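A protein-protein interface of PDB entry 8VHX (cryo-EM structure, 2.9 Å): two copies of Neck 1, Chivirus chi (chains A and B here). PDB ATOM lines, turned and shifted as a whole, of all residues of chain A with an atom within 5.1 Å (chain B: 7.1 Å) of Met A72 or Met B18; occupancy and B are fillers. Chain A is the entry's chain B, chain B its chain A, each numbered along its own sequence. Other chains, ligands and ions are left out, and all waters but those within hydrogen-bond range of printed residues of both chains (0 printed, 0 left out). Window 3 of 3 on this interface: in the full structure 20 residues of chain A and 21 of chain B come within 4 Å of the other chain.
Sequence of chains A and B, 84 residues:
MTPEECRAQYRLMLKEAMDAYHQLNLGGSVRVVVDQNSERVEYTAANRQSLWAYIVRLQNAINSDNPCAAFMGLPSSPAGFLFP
Tyr A54 touches Tyr B21.
Trp B52 touches Arg A57 (CZ2 to CZ, 3.5 Å).
CE of Met A72 touches SD of Met B18, at 3.9 Å.
Met A72 touches Trp B52.
Met A72 touches Ile B55 (SD to CG2, 3.4 Å).
Val B56 touches Leu A74.
Leu A74 touches Gln B59.
The guanidinium group (NE) of Arg A57 is in hydrogen-bond range of the backbone carbonyl oxygen (O) of Phe A71 (2.5 Å).
The guanidinium group of Arg A57 sits at hydrogen-bond distance from the backbone carbonyl oxygen of Met A72 (3.0 Å).
The side-chain amide nitrogen (ND2) of Asn B25 sits at hydrogen-bond distance from the backbone carbonyl oxygen (O) of Tyr B21 (2.7 Å).
Of the printed residues of chain B, Arg A57 touches Trp B52 (3.5 Å).
Cys A68 touches none of the printed residues of chain B.
Met A72 touches just these residues of chain B: Met B18 (3.9 Å), Trp B52 (3.3 Å) and Ile B55 (3.4 Å).
Of the printed residues of chain A, Tyr B21 touches Tyr A54 (3.8 Å).
Printed residues of chain A within 4 Å of Trp B52: Arg A57 (3.5 Å) and Met A72 (3.3 Å).
Of the printed residues of chain A, Val B56 touches Leu A74 (3.6 Å).
The nearest printed residue of chain A that does not touch Ile B55 is Leu A74 (5.6 Å).
Printed residues of chain B that touch a printed residue of chain A: Met B18, Tyr B21, His B22, Trp B52, Ile B55, Val B56 and Gln B59.
Hydrophobic or aromatic side chains of chain B that line the printed part of chain A: Met B18, Tyr B21, His B22, Trp B52, Ile B55 and Val B56.
Along chain A the printed residues that touch a printed residue of chain B span positions 54 to 74.
Among the printed residues, 8 pairs touch across the chains.
The side-chain hydroxyl of Tyr A54 is in hydrogen-bond range of a ring nitrogen (ND1) of His B22 (2.5 Å).
No position is printed for both chains.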
ATOM      1  N   TYR A  10      16.057 -39.592 -24.765  1.00  0.00           N
ATOM      2  CA  TYR A  10      14.655 -39.752 -25.119  1.00  0.00           C
ATOM      3  C   TYR A  10      14.133 -41.145 -24.805  1.00  0.00           C
ATOM      4  O   TYR A  10      12.963 -41.283 -24.452  1.00  0.00           O
ATOM      5  CB  TYR A  10      14.433 -39.433 -26.592  1.00  0.00           C
ATOM      6  CG  TYR A  10      14.722 -38.005 -26.959  1.00  0.00           C
ATOM      7  CD1 TYR A  10      14.406 -36.974 -26.098  1.00  0.00           C
ATOM      8  CD2 TYR A  10      15.244 -37.678 -28.190  1.00  0.00           C
ATOM      9  CE1 TYR A  10      14.653 -35.675 -26.425  1.00  0.00           C
ATOM     10  CE2 TYR A  10      15.486 -36.378 -28.529  1.00  0.00           C
ATOM     11  CZ  TYR A  10      15.186 -35.377 -27.640  1.00  0.00           C
ATOM     12  OH  TYR A  10      15.419 -34.063 -27.957  1.00  0.00           O
ATOM     13  N   TYR A  54       3.033 -37.052 -26.639  1.00  0.00           N
ATOM     14  CA  TYR A  54       4.411 -36.893 -26.201  1.00  0.00           C
ATOM     15  C   TYR A  54       5.188 -38.185 -26.386  1.00  0.00           C
ATOM     16  O   TYR A  54       6.333 -38.175 -26.857  1.00  0.00           O
ATOM     17  CB  TYR A  54       4.408 -36.442 -24.746  1.00  0.00           C
ATOM     18  CG  TYR A  54       5.736 -36.117 -24.141  1.00  0.00           C
ATOM     19  CD1 TYR A  54       6.516 -35.095 -24.631  1.00  0.00           C
ATOM     20  CD2 TYR A  54       6.184 -36.802 -23.036  1.00  0.00           C
ATOM     21  CE1 TYR A  54       7.713 -34.798 -24.061  1.00  0.00           C
ATOM     22  CE2 TYR A  54       7.373 -36.508 -22.467  1.00  0.00           C
ATOM     23  CZ  TYR A  54       8.138 -35.509 -22.977  1.00  0.00           C
ATOM     24  OH  TYR A  54       9.338 -35.219 -22.386  1.00  0.00           O
ATOM     25  N   ARG A  57       6.022 -38.355 -29.981  1.00  0.00           N
ATOM     26  CA  ARG A  57       7.175 -37.518 -30.296  1.00  0.00           C
ATOM     27  C   ARG A  57       8.462 -38.245 -29.967  1.00  0.00           C
ATOM     28  O   ARG A  57       9.392 -38.301 -30.780  1.00  0.00           O
ATOM     29  CB  ARG A  57       7.155 -36.214 -29.508  1.00  0.00           C
ATOM     30  CG  ARG A  57       5.978 -35.312 -29.667  1.00  0.00           C
ATOM     31  CD  ARG A  57       6.437 -33.896 -29.396  1.00  0.00           C
ATOM     32  NE  ARG A  57       7.108 -33.330 -30.553  1.00  0.00           N
ATOM     33  CZ  ARG A  57       6.530 -32.523 -31.431  1.00  0.00           C
ATOM     34  NH1 ARG A  57       7.219 -32.071 -32.456  1.00  0.00           N
ATOM     35  NH2 ARG A  57       5.275 -32.149 -31.281  1.00  0.00           N
ATOM     36  N   PRO A  67      17.612 -37.207 -33.578  1.00  0.00           N
ATOM     37  CA  PRO A  67      16.515 -37.083 -32.613  1.00  0.00           C
ATOM     38  C   PRO A  67      16.204 -35.661 -32.197  1.00  0.00           C
ATOM     39  O   PRO A  67      15.045 -35.240 -32.275  1.00  0.00           O
ATOM     40  CB  PRO A  67      17.017 -37.908 -31.429  1.00  0.00           C
ATOM     41  CG  PRO A  67      17.988 -38.846 -32.003  1.00  0.00           C
ATOM     42  CD  PRO A  67      18.620 -38.182 -33.152  1.00  0.00           C
ATOM     43  N   CYS A  68      17.209 -34.900 -31.769  1.00  0.00           N
ATOM     44  CA  CYS A  68      16.940 -33.570 -31.242  1.00  0.00           C
ATOM     45  C   CYS A  68      16.160 -32.730 -32.239  1.00  0.00           C
ATOM     46  O   CYS A  68      15.398 -31.840 -31.845  1.00  0.00           O
ATOM     47  CB  CYS A  68      18.248 -32.874 -30.886  1.00  0.00           C
ATOM     48  SG  CYS A  68      19.095 -33.536 -29.441  1.00  0.00           S
ATOM     49  N   ALA A  69      16.343 -32.995 -33.529  1.00  0.00           N
ATOM     50  CA  ALA A  69      15.652 -32.248 -34.566  1.00  0.00           C
ATOM     51  C   ALA A  69      14.267 -32.811 -34.841  1.00  0.00           C
ATOM     52  O   ALA A  69      13.351 -32.061 -35.188  1.00  0.00           O
ATOM     53  CB  ALA A  69      16.489 -32.254 -35.835  1.00  0.00           C
ATOM     54  N   ALA A  70      14.101 -34.126 -34.722  1.00  0.00           N
ATOM     55  CA  ALA A  70      12.812 -34.746 -34.997  1.00  0.00           C
ATOM     56  C   ALA A  70      11.837 -34.578 -33.845  1.00  0.00           C
ATOM     57  O   ALA A  70      10.620 -34.617 -34.053  1.00  0.00           O
ATOM     58  CB  ALA A  70      12.998 -36.227 -35.300  1.00  0.00           C
ATOM     59  N   PHE A  71      12.348 -34.404 -32.632  1.00  0.00           N
ATOM     60  CA  PHE A  71      11.479 -34.202 -31.483  1.00  0.00           C
ATOM     61  C   PHE A  71      10.650 -32.939 -31.643  1.00  0.00           C
ATOM     62  O   PHE A  71       9.429 -32.951 -31.452  1.00  0.00           O
ATOM     63  CB  PHE A  71      12.321 -34.127 -30.220  1.00  0.00           C
ATOM     64  CG  PHE A  71      11.540 -33.857 -28.984  1.00  0.00           C
ATOM     65  CD1 PHE A  71      10.958 -34.885 -28.283  1.00  0.00           C
ATOM     66  CD2 PHE A  71      11.389 -32.575 -28.517  1.00  0.00           C
ATOM     67  CE1 PHE A  71      10.247 -34.635 -27.151  1.00  0.00           C
ATOM     68  CE2 PHE A  71      10.679 -32.328 -27.387  1.00  0.00           C
ATOM     69  CZ  PHE A  71      10.107 -33.355 -26.703  1.00  0.00           C
ATOM     70  N   MET A  72      11.302 -31.835 -31.990  1.00  0.00           N
ATOM     71  CA  MET A  72      10.610 -30.564 -32.135  1.00  0.00           C
ATOM     72  C   MET A  72       9.900 -30.463 -33.478  1.00  0.00           C
ATOM     73  O   MET A  72       8.845 -29.829 -33.581  1.00  0.00           O
ATOM     74  CB  MET A  72      11.603 -29.424 -31.969  1.00  0.00           C
ATOM     75  CG  MET A  72      11.061 -28.246 -31.193  1.00  0.00           C
ATOM     76  SD  MET A  72      11.066 -28.538 -29.424  1.00  0.00           S
ATOM     77  CE  MET A  72      12.817 -28.655 -29.122  1.00  0.00           C
ATOM     78  N   GLY A  73      10.463 -31.076 -34.515  1.00  0.00           N
ATOM     79  CA  GLY A  73       9.861 -31.065 -35.833  1.00  0.00           C
ATOM     80  C   GLY A  73       9.929 -29.749 -36.567  1.00  0.00           C
ATOM     81  O   GLY A  73       9.274 -29.603 -37.599  1.00  0.00           O
ATOM     82  N   LEU A  74      10.705 -28.796 -36.077  1.00  0.00           N
ATOM     83  CA  LEU A  74      10.768 -27.454 -36.641  1.00  0.00           C
ATOM     84  C   LEU A  74      11.276 -27.419 -38.076  1.00  0.00           C
ATOM     85  O   LEU A  74      10.958 -26.477 -38.811  1.00  0.00           O
ATOM     86  CB  LEU A  74      11.631 -26.554 -35.770  1.00  0.00           C
ATOM     87  CG  LEU A  74      11.000 -26.247 -34.414  1.00  0.00           C
ATOM     88  CD1 LEU A  74      11.808 -25.191 -33.670  1.00  0.00           C
ATOM     89  CD2 LEU A  74       9.549 -25.819 -34.579  1.00  0.00           C
ATOM     90  N   LEU B  12      19.416 -22.065 -21.823  1.00  0.00           N
ATOM     91  CA  LEU B  12      19.089 -22.453 -20.456  1.00  0.00           C
ATOM     92  C   LEU B  12      17.584 -22.418 -20.228  1.00  0.00           C
ATOM     93  O   LEU B  12      17.012 -23.322 -19.596  1.00  0.00           O
ATOM     94  CB  LEU B  12      19.803 -21.534 -19.472  1.00  0.00           C
ATOM     95  CG  LEU B  12      21.326 -21.588 -19.497  1.00  0.00           C
ATOM     96  CD1 LEU B  12      21.888 -20.512 -18.605  1.00  0.00           C
ATOM     97  CD2 LEU B  12      21.842 -22.946 -19.071  1.00  0.00           C
ATOM     98  N   MET B  13      16.924 -21.390 -20.755  1.00  0.00           N
ATOM     99  CA  MET B  13      15.479 -21.295 -20.613  1.00  0.00           C
ATOM    100  C   MET B  13      14.786 -22.457 -21.307  1.00  0.00           C
ATOM    101  O   MET B  13      13.774 -22.968 -20.822  1.00  0.00           O
ATOM    102  CB  MET B  13      15.001 -19.965 -21.174  1.00  0.00           C
ATOM    103  CG  MET B  13      15.507 -18.770 -20.422  1.00  0.00           C
ATOM    104  SD  MET B  13      15.464 -17.280 -21.404  1.00  0.00           S
ATOM    105  CE  MET B  13      13.712 -17.047 -21.456  1.00  0.00           C
ATOM    106  N   LEU B  14      15.329 -22.892 -22.440  1.00  0.00           N
ATOM    107  CA  LEU B  14      14.781 -24.034 -23.154  1.00  0.00           C
ATOM    108  C   LEU B  14      14.968 -25.320 -22.374  1.00  0.00           C
ATOM    109  O   LEU B  14      14.081 -26.177 -22.359  1.00  0.00           O
ATOM    110  CB  LEU B  14      15.443 -24.151 -24.514  1.00  0.00           C
ATOM    111  CG  LEU B  14      15.028 -25.351 -25.338  1.00  0.00           C
ATOM    112  CD1 LEU B  14      13.658 -25.135 -25.843  1.00  0.00           C
ATOM    113  CD2 LEU B  14      15.966 -25.538 -26.469  1.00  0.00           C
ATOM    114  N   LYS B  15      16.135 -25.504 -21.764  1.00  0.00           N
ATOM    115  CA  LYS B  15      16.305 -26.637 -20.869  1.00  0.00           C
ATOM    116  C   LYS B  15      15.193 -26.664 -19.827  1.00  0.00           C
ATOM    117  O   LYS B  15      14.500 -27.678 -19.657  1.00  0.00           O
ATOM    118  CB  LYS B  15      17.671 -26.571 -20.198  1.00  0.00           C
ATOM    119  CG  LYS B  15      18.665 -27.621 -20.656  1.00  0.00           C
ATOM    120  CD  LYS B  15      19.024 -27.479 -22.125  1.00  0.00           C
ATOM    121  CE  LYS B  15      20.061 -28.518 -22.536  1.00  0.00           C
ATOM    122  NZ  LYS B  15      20.430 -28.443 -23.979  1.00  0.00           N
ATOM    123  N   GLU B  16      14.992 -25.541 -19.137  1.00  0.00           N
ATOM    124  CA  GLU B  16      13.965 -25.502 -18.101  1.00  0.00           C
ATOM    125  C   GLU B  16      12.586 -25.778 -18.680  1.00  0.00           C
ATOM    126  O   GLU B  16      11.778 -26.489 -18.072  1.00  0.00           O
ATOM    127  CB  GLU B  16      13.966 -24.155 -17.388  1.00  0.00           C
ATOM    128  CG  GLU B  16      15.304 -23.705 -16.872  1.00  0.00           C
ATOM    129  CD  GLU B  16      15.187 -22.607 -15.839  1.00  0.00           C
ATOM    130  OE1 GLU B  16      15.215 -21.421 -16.225  1.00  0.00           O
ATOM    131  OE2 GLU B  16      15.074 -22.931 -14.640  1.00  0.00           O
ATOM    132  N   ALA B  17      12.306 -25.246 -19.865  1.00  0.00           N
ATOM    133  CA  ALA B  17      10.968 -25.351 -20.421  1.00  0.00           C
ATOM    134  C   ALA B  17      10.676 -26.764 -20.899  1.00  0.00           C
ATOM    135  O   ALA B  17       9.564 -27.268 -20.731  1.00  0.00           O
ATOM    136  CB  ALA B  17      10.801 -24.352 -21.551  1.00  0.00           C
ATOM    137  N   MET B  18      11.658 -27.421 -21.507  1.00  0.00           N
ATOM    138  CA  MET B  18      11.447 -28.792 -21.936  1.00  0.00           C
ATOM    139  C   MET B  18      11.326 -29.731 -20.748  1.00  0.00           C
ATOM    140  O   MET B  18      10.530 -30.675 -20.784  1.00  0.00           O
ATOM    141  CB  MET B  18      12.576 -29.231 -22.854  1.00  0.00           C
ATOM    142  CG  MET B  18      12.388 -28.845 -24.293  1.00  0.00           C
ATOM    143  SD  MET B  18      13.746 -29.349 -25.352  1.00  0.00           S
ATOM    144  CE  MET B  18      13.736 -31.113 -25.059  1.00  0.00           C
ATOM    145  N   ASP B  19      12.078 -29.482 -19.676  1.00  0.00           N
ATOM    146  CA  ASP B  19      11.888 -30.274 -18.468  1.00  0.00           C
ATOM    147  C   ASP B  19      10.495 -30.064 -17.898  1.00  0.00           C
ATOM    148  O   ASP B  19       9.847 -31.013 -17.439  1.00  0.00           O
ATOM    149  CB  ASP B  19      12.948 -29.916 -17.436  1.00  0.00           C
ATOM    150  CG  ASP B  19      14.354 -30.109 -17.959  1.00  0.00           C
ATOM    151  OD1 ASP B  19      15.313 -29.822 -17.214  1.00  0.00           O
ATOM    152  OD2 ASP B  19      14.505 -30.547 -19.117  1.00  0.00           O
ATOM    153  N   ALA B  20      10.019 -28.825 -17.923  1.00  0.00           N
ATOM    154  CA  ALA B  20       8.675 -28.532 -17.454  1.00  0.00           C
ATOM    155  C   ALA B  20       7.624 -29.221 -18.307  1.00  0.00           C
ATOM    156  O   ALA B  20       6.621 -29.713 -17.788  1.00  0.00           O
ATOM    157  CB  ALA B  20       8.458 -27.032 -17.463  1.00  0.00           C
ATOM    158  N   TYR B  21       7.832 -29.260 -19.619  1.00  0.00           N
ATOM    159  CA  TYR B  21       6.886 -29.913 -20.512  1.00  0.00           C
ATOM    160  C   TYR B  21       6.848 -31.412 -20.275  1.00  0.00           C
ATOM    161  O   TYR B  21       5.768 -32.021 -20.257  1.00  0.00           O
ATOM    162  CB  TYR B  21       7.280 -29.602 -21.946  1.00  0.00           C
ATOM    163  CG  TYR B  21       6.303 -30.017 -22.997  1.00  0.00           C
ATOM    164  CD1 TYR B  21       5.092 -29.376 -23.138  1.00  0.00           C
ATOM    165  CD2 TYR B  21       6.609 -31.029 -23.879  1.00  0.00           C
ATOM    166  CE1 TYR B  21       4.209 -29.750 -24.101  1.00  0.00           C
ATOM    167  CE2 TYR B  21       5.731 -31.407 -24.843  1.00  0.00           C
ATOM    168  CZ  TYR B  21       4.531 -30.764 -24.956  1.00  0.00           C
ATOM    169  OH  TYR B  21       3.639 -31.140 -25.927  1.00  0.00           O
ATOM    170  N   HIS B  22       8.014 -32.009 -20.061  1.00  0.00           N
ATOM    171  CA  HIS B  22       8.077 -33.402 -19.658  1.00  0.00           C
ATOM    172  C   HIS B  22       7.255 -33.633 -18.406  1.00  0.00           C
ATOM    173  O   HIS B  22       6.314 -34.432 -18.404  1.00  0.00           O
ATOM    174  CB  HIS B  22       9.528 -33.782 -19.421  1.00  0.00           C
ATOM    175  CG  HIS B  22       9.744 -35.231 -19.147  1.00  0.00           C
ATOM    176  ND1 HIS B  22       9.591 -36.198 -20.112  1.00  0.00           N
ATOM    177  CD2 HIS B  22      10.106 -35.879 -18.018  1.00  0.00           C
ATOM    178  CE1 HIS B  22       9.849 -37.382 -19.589  1.00  0.00           C
ATOM    179  NE2 HIS B  22      10.163 -37.215 -18.319  1.00  0.00           N
ATOM    180  N   GLN B  23       7.578 -32.917 -17.335  1.00  0.00           N
ATOM    181  CA  GLN B  23       6.872 -33.119 -16.077  1.00  0.00           C
ATOM    182  C   GLN B  23       5.384 -32.842 -16.221  1.00  0.00           C
ATOM    183  O   GLN B  23       4.563 -33.440 -15.519  1.00  0.00           O
ATOM    184  CB  GLN B  23       7.481 -32.241 -14.991  1.00  0.00           C
ATOM    185  CG  GLN B  23       8.884 -32.624 -14.581  1.00  0.00           C
ATOM    186  CD  GLN B  23       9.015 -34.078 -14.206  1.00  0.00           C
ATOM    187  OE1 GLN B  23       9.655 -34.854 -14.910  1.00  0.00           O
ATOM    188  NE2 GLN B  23       8.406 -34.460 -13.097  1.00  0.00           N
ATOM    189  N   LEU B  24       5.017 -31.935 -17.120  1.00  0.00           N
ATOM    190  CA  LEU B  24       3.622 -31.554 -17.290  1.00  0.00           C
ATOM    191  C   LEU B  24       2.815 -32.654 -17.942  1.00  0.00           C
ATOM    192  O   LEU B  24       1.707 -32.967 -17.493  1.00  0.00           O
ATOM    193  CB  LEU B  24       3.546 -30.291 -18.131  1.00  0.00           C
ATOM    194  CG  LEU B  24       2.171 -29.728 -18.438  1.00  0.00           C
ATOM    195  CD1 LEU B  24       1.441 -29.320 -17.210  1.00  0.00           C
ATOM    196  CD2 LEU B  24       2.343 -28.569 -19.341  1.00  0.00           C
ATOM    197  N   ASN B  25       3.340 -33.246 -19.010  1.00  0.00           N
ATOM    198  CA  ASN B  25       2.597 -34.304 -19.675  1.00  0.00           C
ATOM    199  C   ASN B  25       2.537 -35.556 -18.819  1.00  0.00           C
ATOM    200  O   ASN B  25       1.541 -36.285 -18.848  1.00  0.00           O
ATOM    201  CB  ASN B  25       3.223 -34.591 -21.020  1.00  0.00           C
ATOM    202  CG  ASN B  25       2.959 -33.501 -22.004  1.00  0.00           C
ATOM    203  OD1 ASN B  25       1.877 -33.395 -22.568  1.00  0.00           O
ATOM    204  ND2 ASN B  25       3.935 -32.644 -22.178  1.00  0.00           N
ATOM    205  N   LEU B  51       3.085 -23.662 -23.528  1.00  0.00           N
ATOM    206  CA  LEU B  51       4.440 -24.068 -23.198  1.00  0.00           C
ATOM    207  C   LEU B  51       5.157 -24.633 -24.410  1.00  0.00           C
ATOM    208  O   LEU B  51       6.336 -24.340 -24.632  1.00  0.00           O
ATOM    209  CB  LEU B  51       4.393 -25.073 -22.065  1.00  0.00           C
ATOM    210  CG  LEU B  51       5.702 -25.602 -21.525  1.00  0.00           C
ATOM    211  CD1 LEU B  51       6.671 -24.517 -21.330  1.00  0.00           C
ATOM    212  CD2 LEU B  51       5.441 -26.228 -20.221  1.00  0.00           C
ATOM    213  N   TRP B  52       4.463 -25.419 -25.223  1.00  0.00           N
ATOM    214  CA  TRP B  52       5.070 -25.879 -26.460  1.00  0.00           C
ATOM    215  C   TRP B  52       5.402 -24.708 -27.369  1.00  0.00           C
ATOM    216  O   TRP B  52       6.464 -24.672 -27.998  1.00  0.00           O
ATOM    217  CB  TRP B  52       4.144 -26.864 -27.156  1.00  0.00           C
ATOM    218  CG  TRP B  52       4.715 -27.422 -28.369  1.00  0.00           C
ATOM    219  CD1 TRP B  52       4.248 -27.270 -29.626  1.00  0.00           C
ATOM    220  CD2 TRP B  52       5.900 -28.203 -28.469  1.00  0.00           C
ATOM    221  NE1 TRP B  52       5.059 -27.918 -30.510  1.00  0.00           N
ATOM    222  CE2 TRP B  52       6.086 -28.499 -29.822  1.00  0.00           C
ATOM    223  CE3 TRP B  52       6.821 -28.684 -27.543  1.00  0.00           C
ATOM    224  CZ2 TRP B  52       7.146 -29.249 -30.274  1.00  0.00           C
ATOM    225  CZ3 TRP B  52       7.873 -29.429 -27.994  1.00  0.00           C
ATOM    226  CH2 TRP B  52       8.028 -29.708 -29.343  1.00  0.00           C
ATOM    227  N   ILE B  55       8.489 -23.041 -26.138  1.00  0.00           N
ATOM    228  CA  ILE B  55       9.620 -23.871 -26.527  1.00  0.00           C
ATOM    229  C   ILE B  55       9.988 -23.627 -27.980  1.00  0.00           C
ATOM    230  O   ILE B  55      11.167 -23.601 -28.345  1.00  0.00           O
ATOM    231  CB  ILE B  55       9.287 -25.346 -26.270  1.00  0.00           C
ATOM    232  CG1 ILE B  55       9.387 -25.634 -24.791  1.00  0.00           C
ATOM    233  CG2 ILE B  55      10.201 -26.224 -27.016  1.00  0.00           C
ATOM    234  CD1 ILE B  55       8.730 -26.864 -24.394  1.00  0.00           C
ATOM    235  N   VAL B  56       8.985 -23.466 -28.833  1.00  0.00           N
ATOM    236  CA  VAL B  56       9.252 -23.247 -30.247  1.00  0.00           C
ATOM    237  C   VAL B  56       9.838 -21.862 -30.480  1.00  0.00           C
ATOM    238  O   VAL B  56      10.749 -21.695 -31.297  1.00  0.00           O
ATOM    239  CB  VAL B  56       7.979 -23.467 -31.068  1.00  0.00           C
ATOM    240  CG1 VAL B  56       8.265 -23.217 -32.489  1.00  0.00           C
ATOM    241  CG2 VAL B  56       7.505 -24.857 -30.910  1.00  0.00           C
ATOM    242  N   LEU B  58      11.741 -20.305 -28.404  1.00  0.00           N
ATOM    243  CA  LEU B  58      13.114 -20.385 -27.936  1.00  0.00           C
ATOM    244  C   LEU B  58      13.991 -21.118 -28.935  1.00  0.00           C
ATOM    245  O   LEU B  58      15.066 -20.637 -29.302  1.00  0.00           O
ATOM    246  CB  LEU B  58      13.157 -21.083 -26.591  1.00  0.00           C
ATOM    247  CG  LEU B  58      12.468 -20.377 -25.439  1.00  0.00           C
ATOM    248  CD1 LEU B  58      12.355 -21.282 -24.271  1.00  0.00           C
ATOM    249  CD2 LEU B  58      13.224 -19.182 -25.050  1.00  0.00           C
ATOM    250  N   GLN B  59      13.559 -22.298 -29.368  1.00  0.00           N
ATOM    251  CA  GLN B  59      14.348 -23.053 -30.330  1.00  0.00           C
ATOM    252  C   GLN B  59      14.555 -22.262 -31.609  1.00  0.00           C
ATOM    253  O   GLN B  59      15.633 -22.315 -32.209  1.00  0.00           O
ATOM    254  CB  GLN B  59      13.684 -24.390 -30.626  1.00  0.00           C
ATOM    255  CG  GLN B  59      14.441 -25.243 -31.616  1.00  0.00           C
ATOM    256  CD  GLN B  59      15.811 -25.661 -31.134  1.00  0.00           C
ATOM    257  OE1 GLN B  59      16.767 -25.697 -31.906  1.00  0.00           O
ATOM    258  NE2 GLN B  59      15.913 -26.001 -29.862  1.00  0.00           N
